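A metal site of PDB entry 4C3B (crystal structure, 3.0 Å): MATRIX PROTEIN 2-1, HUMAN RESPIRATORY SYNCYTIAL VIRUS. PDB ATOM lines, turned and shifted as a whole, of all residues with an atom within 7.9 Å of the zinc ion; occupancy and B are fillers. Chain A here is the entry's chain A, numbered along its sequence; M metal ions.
The side-chain sulfur (SG) of Cys 12 lies close to the backbone NH (N) of Glu 15 (3.5 Å). O of Ser 29 lies within hydrogen-bond range of N of Cys 12, at 3.1 Å. The side-chain sulfur (SG) of Cys 26 sits close to the backbone NH (N) of Phe 28 (3.7 Å). The backbone NH of Cys 20 sits at hydrogen-bond distance from the side-chain carboxylate of Glu 15, at 3.0 Å. SG of Cys 20 sits close to N of Asn 22. A ring nitrogen (ND1) of His 30 lies close to the backbone carbonyl oxygen (O) of Phe 28 (3.0 Å). The side-chain sulfur (SG) of Cys 12 sits close to the backbone NH (N) of Phe 14.
The nearest printed residue that does not touch the zinc ion is Phe 28 (4.4 Å).
The zinc ion is bound by the side-chain sulfur (SG) of Cys 26, the side-chain sulfur (SG) of Cys 12, a ring nitrogen (NE2) of His 30 and the side-chain sulfur (SG) of Cys 20. The zinc ion has four donor atoms within binding distance.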
ATOM      1  N   ASN A  10     -29.342 -14.199 -27.798  1.00  0.00           N
ATOM      2  CA  ASN A  10     -29.300 -14.019 -26.362  1.00  0.00           C
ATOM      3  C   ASN A  10     -27.919 -14.197 -25.734  1.00  0.00           C
ATOM      4  O   ASN A  10     -27.022 -14.839 -26.300  1.00  0.00           O
ATOM      5  CB  ASN A  10     -30.202 -14.997 -25.706  1.00  0.00           C
ATOM      6  CG  ASN A  10     -31.640 -14.721 -26.002  1.00  0.00           C
ATOM      7  OD1 ASN A  10     -32.106 -13.588 -25.884  1.00  0.00           O
ATOM      8  ND2 ASN A  10     -32.377 -15.758 -26.309  1.00  0.00           N
ATOM      9  N   PRO A  11     -27.733 -13.627 -24.559  1.00  0.00           N
ATOM     10  CA  PRO A  11     -26.433 -13.692 -23.966  1.00  0.00           C
ATOM     11  C   PRO A  11     -26.082 -15.086 -23.508  1.00  0.00           C
ATOM     12  O   PRO A  11     -26.857 -15.702 -22.808  1.00  0.00           O
ATOM     13  CB  PRO A  11     -26.537 -12.741 -22.762  1.00  0.00           C
ATOM     14  CG  PRO A  11     -27.958 -12.320 -22.688  1.00  0.00           C
ATOM     15  CD  PRO A  11     -28.544 -12.533 -24.031  1.00  0.00           C
ATOM     16  N   CYS A  12     -24.875 -15.527 -23.827  1.00  0.00           N
ATOM     17  CA  CYS A  12     -24.330 -16.772 -23.289  1.00  0.00           C
ATOM     18  C   CYS A  12     -24.298 -16.808 -21.771  1.00  0.00           C
ATOM     19  O   CYS A  12     -23.538 -16.063 -21.142  1.00  0.00           O
ATOM     20  CB  CYS A  12     -22.885 -16.969 -23.800  1.00  0.00           C
ATOM     21  SG  CYS A  12     -22.021 -18.414 -23.161  1.00  0.00           S
ATOM     22  N   LYS A  13     -25.062 -17.738 -21.190  1.00  0.00           N
ATOM     23  CA  LYS A  13     -25.130 -17.902 -19.729  1.00  0.00           C
ATOM     24  C   LYS A  13     -23.787 -18.340 -19.148  1.00  0.00           C
ATOM     25  O   LYS A  13     -23.536 -18.068 -18.006  1.00  0.00           O
ATOM     26  CB  LYS A  13     -26.249 -18.848 -19.343  1.00  0.00           C
ATOM     27  CG  LYS A  13     -27.627 -18.239 -19.568  1.00  0.00           C
ATOM     28  CD  LYS A  13     -28.796 -19.214 -19.413  1.00  0.00           C
ATOM     29  CE  LYS A  13     -28.967 -19.747 -17.974  1.00  0.00           C
ATOM     30  NZ  LYS A  13     -29.077 -18.728 -16.885  1.00  0.00           N
ATOM     31  N   PHE A  14     -22.910 -18.975 -19.910  1.00  0.00           N
ATOM     32  CA  PHE A  14     -21.596 -19.289 -19.387  1.00  0.00           C
ATOM     33  C   PHE A  14     -20.756 -18.036 -19.189  1.00  0.00           C
ATOM     34  O   PHE A  14     -20.036 -17.946 -18.207  1.00  0.00           O
ATOM     35  CB  PHE A  14     -20.823 -20.247 -20.320  1.00  0.00           C
ATOM     36  CG  PHE A  14     -21.344 -21.650 -20.295  1.00  0.00           C
ATOM     37  CD1 PHE A  14     -22.426 -22.013 -21.087  1.00  0.00           C
ATOM     38  CD2 PHE A  14     -20.765 -22.579 -19.451  1.00  0.00           C
ATOM     39  CE1 PHE A  14     -22.944 -23.279 -21.032  1.00  0.00           C
ATOM     40  CE2 PHE A  14     -21.256 -23.852 -19.388  1.00  0.00           C
ATOM     41  CZ  PHE A  14     -22.353 -24.189 -20.178  1.00  0.00           C
ATOM     42  N   GLU A  15     -20.853 -17.118 -20.170  1.00  0.00           N
ATOM     43  CA  GLU A  15     -20.156 -15.807 -20.181  1.00  0.00           C
ATOM     44  C   GLU A  15     -20.721 -14.914 -19.132  1.00  0.00           C
ATOM     45  O   GLU A  15     -19.993 -14.190 -18.481  1.00  0.00           O
ATOM     46  CB  GLU A  15     -20.360 -15.086 -21.524  1.00  0.00           C
ATOM     47  CG  GLU A  15     -19.533 -13.818 -21.732  1.00  0.00           C
ATOM     48  CD  GLU A  15     -18.044 -14.081 -21.840  1.00  0.00           C
ATOM     49  OE1 GLU A  15     -17.655 -15.230 -22.161  1.00  0.00           O
ATOM     50  OE2 GLU A  15     -17.239 -13.138 -21.708  1.00  0.00           O
ATOM     51  N   ILE A  16     -22.046 -14.959 -18.957  1.00  0.00           N
ATOM     52  CA  ILE A  16     -22.638 -14.279 -17.801  1.00  0.00           C
ATOM     53  C   ILE A  16     -21.896 -14.618 -16.498  1.00  0.00           C
ATOM     54  O   ILE A  16     -21.758 -13.764 -15.680  1.00  0.00           O
ATOM     55  CB  ILE A  16     -24.124 -14.518 -17.673  1.00  0.00           C
ATOM     56  CG1 ILE A  16     -24.832 -13.955 -18.906  1.00  0.00           C
ATOM     57  CG2 ILE A  16     -24.635 -13.792 -16.462  1.00  0.00           C
ATOM     58  CD1 ILE A  16     -26.363 -13.807 -18.781  1.00  0.00           C
ATOM     59  N   HIS A  19     -16.290 -16.583 -18.153  1.00  0.00           N
ATOM     60  CA  HIS A  19     -15.804 -16.802 -19.492  1.00  0.00           C
ATOM     61  C   HIS A  19     -16.363 -18.081 -20.077  1.00  0.00           C
ATOM     62  O   HIS A  19     -15.957 -19.154 -19.694  1.00  0.00           O
ATOM     63  CB  HIS A  19     -14.279 -16.776 -19.482  1.00  0.00           C
ATOM     64  CG  HIS A  19     -13.721 -15.466 -18.987  1.00  0.00           C
ATOM     65  ND1 HIS A  19     -13.872 -14.290 -19.703  1.00  0.00           N
ATOM     66  CD2 HIS A  19     -13.039 -15.143 -17.858  1.00  0.00           C
ATOM     67  CE1 HIS A  19     -13.276 -13.304 -19.042  1.00  0.00           C
ATOM     68  NE2 HIS A  19     -12.776 -13.795 -17.919  1.00  0.00           N
ATOM     69  N   CYS A  20     -17.269 -17.954 -21.046  1.00  0.00           N
ATOM     70  CA  CYS A  20     -17.679 -19.106 -21.905  1.00  0.00           C
ATOM     71  C   CYS A  20     -16.503 -19.930 -22.446  1.00  0.00           C
ATOM     72  O   CYS A  20     -15.568 -19.383 -22.896  1.00  0.00           O
ATOM     73  CB  CYS A  20     -18.542 -18.630 -23.079  1.00  0.00           C
ATOM     74  SG  CYS A  20     -19.021 -19.960 -24.189  1.00  0.00           S
ATOM     75  N   LEU A  21     -16.526 -21.247 -22.339  1.00  0.00           N
ATOM     76  CA  LEU A  21     -15.350 -22.059 -22.676  1.00  0.00           C
ATOM     77  C   LEU A  21     -15.578 -22.989 -23.851  1.00  0.00           C
ATOM     78  O   LEU A  21     -14.838 -23.947 -24.046  1.00  0.00           O
ATOM     79  CB  LEU A  21     -14.897 -22.882 -21.438  1.00  0.00           C
ATOM     80  CG  LEU A  21     -14.316 -22.143 -20.241  1.00  0.00           C
ATOM     81  CD1 LEU A  21     -13.814 -23.099 -19.137  1.00  0.00           C
ATOM     82  CD2 LEU A  21     -13.192 -21.248 -20.689  1.00  0.00           C
ATOM     83  N   ASN A  22     -16.629 -22.728 -24.602  1.00  0.00           N
ATOM     84  CA  ASN A  22     -17.048 -23.615 -25.668  1.00  0.00           C
ATOM     85  C   ASN A  22     -16.531 -23.157 -27.035  1.00  0.00           C
ATOM     86  O   ASN A  22     -16.991 -23.694 -28.035  1.00  0.00           O
ATOM     87  CB  ASN A  22     -18.565 -23.693 -25.710  1.00  0.00           C
ATOM     88  CG  ASN A  22     -19.127 -24.465 -24.565  1.00  0.00           C
ATOM     89  OD1 ASN A  22     -18.588 -25.496 -24.209  1.00  0.00           O
ATOM     90  ND2 ASN A  22     -20.167 -23.914 -23.908  1.00  0.00           N
ATOM     91  N   GLY A  23     -15.603 -22.191 -27.098  1.00  0.00           N
ATOM     92  CA  GLY A  23     -15.136 -21.708 -28.377  1.00  0.00           C
ATOM     93  C   GLY A  23     -16.248 -21.444 -29.407  1.00  0.00           C
ATOM     94  O   GLY A  23     -17.348 -21.007 -29.053  1.00  0.00           O
ATOM     95  N   ARG A  25     -18.104 -23.243 -31.103  1.00  0.00           N
ATOM     96  CA  ARG A  25     -19.316 -24.099 -31.075  1.00  0.00           C
ATOM     97  C   ARG A  25     -20.501 -23.390 -30.486  1.00  0.00           C
ATOM     98  O   ARG A  25     -21.619 -23.543 -30.962  1.00  0.00           O
ATOM     99  CB  ARG A  25     -19.066 -25.349 -30.278  1.00  0.00           C
ATOM    100  CG  ARG A  25     -17.995 -26.213 -30.896  1.00  0.00           C
ATOM    101  CD  ARG A  25     -16.840 -26.574 -29.952  1.00  0.00           C
ATOM    102  NE  ARG A  25     -17.025 -27.937 -29.453  1.00  0.00           N
ATOM    103  CZ  ARG A  25     -17.384 -28.256 -28.228  1.00  0.00           C
ATOM    104  NH1 ARG A  25     -17.598 -27.321 -27.301  1.00  0.00           N
ATOM    105  NH2 ARG A  25     -17.519 -29.527 -27.911  1.00  0.00           N
ATOM    106  N   CYS A  26     -20.242 -22.544 -29.497  1.00  0.00           N
ATOM    107  CA  CYS A  26     -21.294 -21.795 -28.773  1.00  0.00           C
ATOM    108  C   CYS A  26     -21.930 -20.700 -29.575  1.00  0.00           C
ATOM    109  O   CYS A  26     -21.250 -19.810 -30.044  1.00  0.00           O
ATOM    110  CB  CYS A  26     -20.728 -21.184 -27.515  1.00  0.00           C
ATOM    111  SG  CYS A  26     -21.955 -20.367 -26.488  1.00  0.00           S
ATOM    112  N   HIS A  27     -23.249 -20.774 -29.720  1.00  0.00           N
ATOM    113  CA  HIS A  27     -23.950 -19.889 -30.623  1.00  0.00           C
ATOM    114  C   HIS A  27     -24.737 -18.802 -29.914  1.00  0.00           C
ATOM    115  O   HIS A  27     -25.528 -18.109 -30.501  1.00  0.00           O
ATOM    116  CB  HIS A  27     -24.815 -20.715 -31.561  1.00  0.00           C
ATOM    117  CG  HIS A  27     -24.039 -21.287 -32.711  1.00  0.00           C
ATOM    118  ND1 HIS A  27     -24.148 -22.601 -33.102  1.00  0.00           N
ATOM    119  CD2 HIS A  27     -23.155 -20.702 -33.564  1.00  0.00           C
ATOM    120  CE1 HIS A  27     -23.367 -22.812 -34.153  1.00  0.00           C
ATOM    121  NE2 HIS A  27     -22.750 -21.676 -34.446  1.00  0.00           N
ATOM    122  N   PHE A  28     -24.437 -18.622 -28.644  1.00  0.00           N
ATOM    123  CA  PHE A  28     -24.960 -17.504 -27.903  1.00  0.00           C
ATOM    124  C   PHE A  28     -24.060 -16.269 -28.017  1.00  0.00           C
ATOM    125  O   PHE A  28     -22.859 -16.382 -28.304  1.00  0.00           O
ATOM    126  CB  PHE A  28     -25.061 -17.907 -26.452  1.00  0.00           C
ATOM    127  CG  PHE A  28     -26.195 -18.820 -26.174  1.00  0.00           C
ATOM    128  CD1 PHE A  28     -27.478 -18.330 -26.038  1.00  0.00           C
ATOM    129  CD2 PHE A  28     -25.975 -20.159 -25.965  1.00  0.00           C
ATOM    130  CE1 PHE A  28     -28.539 -19.166 -25.724  1.00  0.00           C
ATOM    131  CE2 PHE A  28     -27.037 -20.988 -25.644  1.00  0.00           C
ATOM    132  CZ  PHE A  28     -28.322 -20.483 -25.525  1.00  0.00           C
ATOM    133  N   SER A  29     -24.615 -15.066 -27.743  1.00  0.00           N
ATOM    134  CA  SER A  29     -23.824 -13.863 -27.840  1.00  0.00           C
ATOM    135  C   SER A  29     -22.725 -13.754 -26.826  1.00  0.00           C
ATOM    136  O   SER A  29     -22.959 -13.964 -25.653  1.00  0.00           O
ATOM    137  CB  SER A  29     -24.676 -12.647 -27.674  1.00  0.00           C
ATOM    138  OG  SER A  29     -23.797 -11.502 -27.752  1.00  0.00           O
ATOM    139  N   HIS A  30     -21.511 -13.433 -27.249  1.00  0.00           N
ATOM    140  CA  HIS A  30     -20.465 -13.048 -26.307  1.00  0.00           C
ATOM    141  C   HIS A  30     -20.014 -11.612 -26.512  1.00  0.00           C
ATOM    142  O   HIS A  30     -18.881 -11.221 -26.155  1.00  0.00           O
ATOM    143  CB  HIS A  30     -19.269 -13.983 -26.397  1.00  0.00           C
ATOM    144  CG  HIS A  30     -19.644 -15.420 -26.391  1.00  0.00           C
ATOM    145  ND1 HIS A  30     -20.021 -16.083 -27.531  1.00  0.00           N
ATOM    146  CD2 HIS A  30     -19.691 -16.326 -25.382  1.00  0.00           C
ATOM    147  CE1 HIS A  30     -20.297 -17.343 -27.230  1.00  0.00           C
ATOM    148  NE2 HIS A  30     -20.098 -17.518 -25.939  1.00  0.00           N
ATOM    149  N   TRP A  35     -25.817  -7.226 -25.564  1.00  0.00           N
ATOM    150  CA  TRP A  35     -26.493  -7.775 -24.395  1.00  0.00           C
ATOM    151  C   TRP A  35     -27.407  -6.773 -23.801  1.00  0.00           C
ATOM    152  O   TRP A  35     -27.154  -5.583 -23.885  1.00  0.00           O
ATOM    153  CB  TRP A  35     -25.479  -8.118 -23.269  1.00  0.00           C
ATOM    154  CG  TRP A  35     -24.672  -9.323 -23.492  1.00  0.00           C
ATOM    155  CD1 TRP A  35     -24.446  -9.910 -24.668  1.00  0.00           C
ATOM    156  CD2 TRP A  35     -23.976 -10.063 -22.524  1.00  0.00           C
ATOM    157  NE1 TRP A  35     -23.667 -11.003 -24.501  1.00  0.00           N
ATOM    158  CE2 TRP A  35     -23.367 -11.123 -23.179  1.00  0.00           C
ATOM    159  CE3 TRP A  35     -23.809  -9.933 -21.162  1.00  0.00           C
ATOM    160  CZ2 TRP A  35     -22.586 -12.046 -22.524  1.00  0.00           C
ATOM    161  CZ3 TRP A  35     -23.065 -10.840 -20.509  1.00  0.00           C
ATOM    162  CH2 TRP A  35     -22.446 -11.888 -21.192  1.00  0.00           C
HETATM  163 ZN    ZN M   1     -21.118 -19.176 -24.977  1.00  0.00          ZN
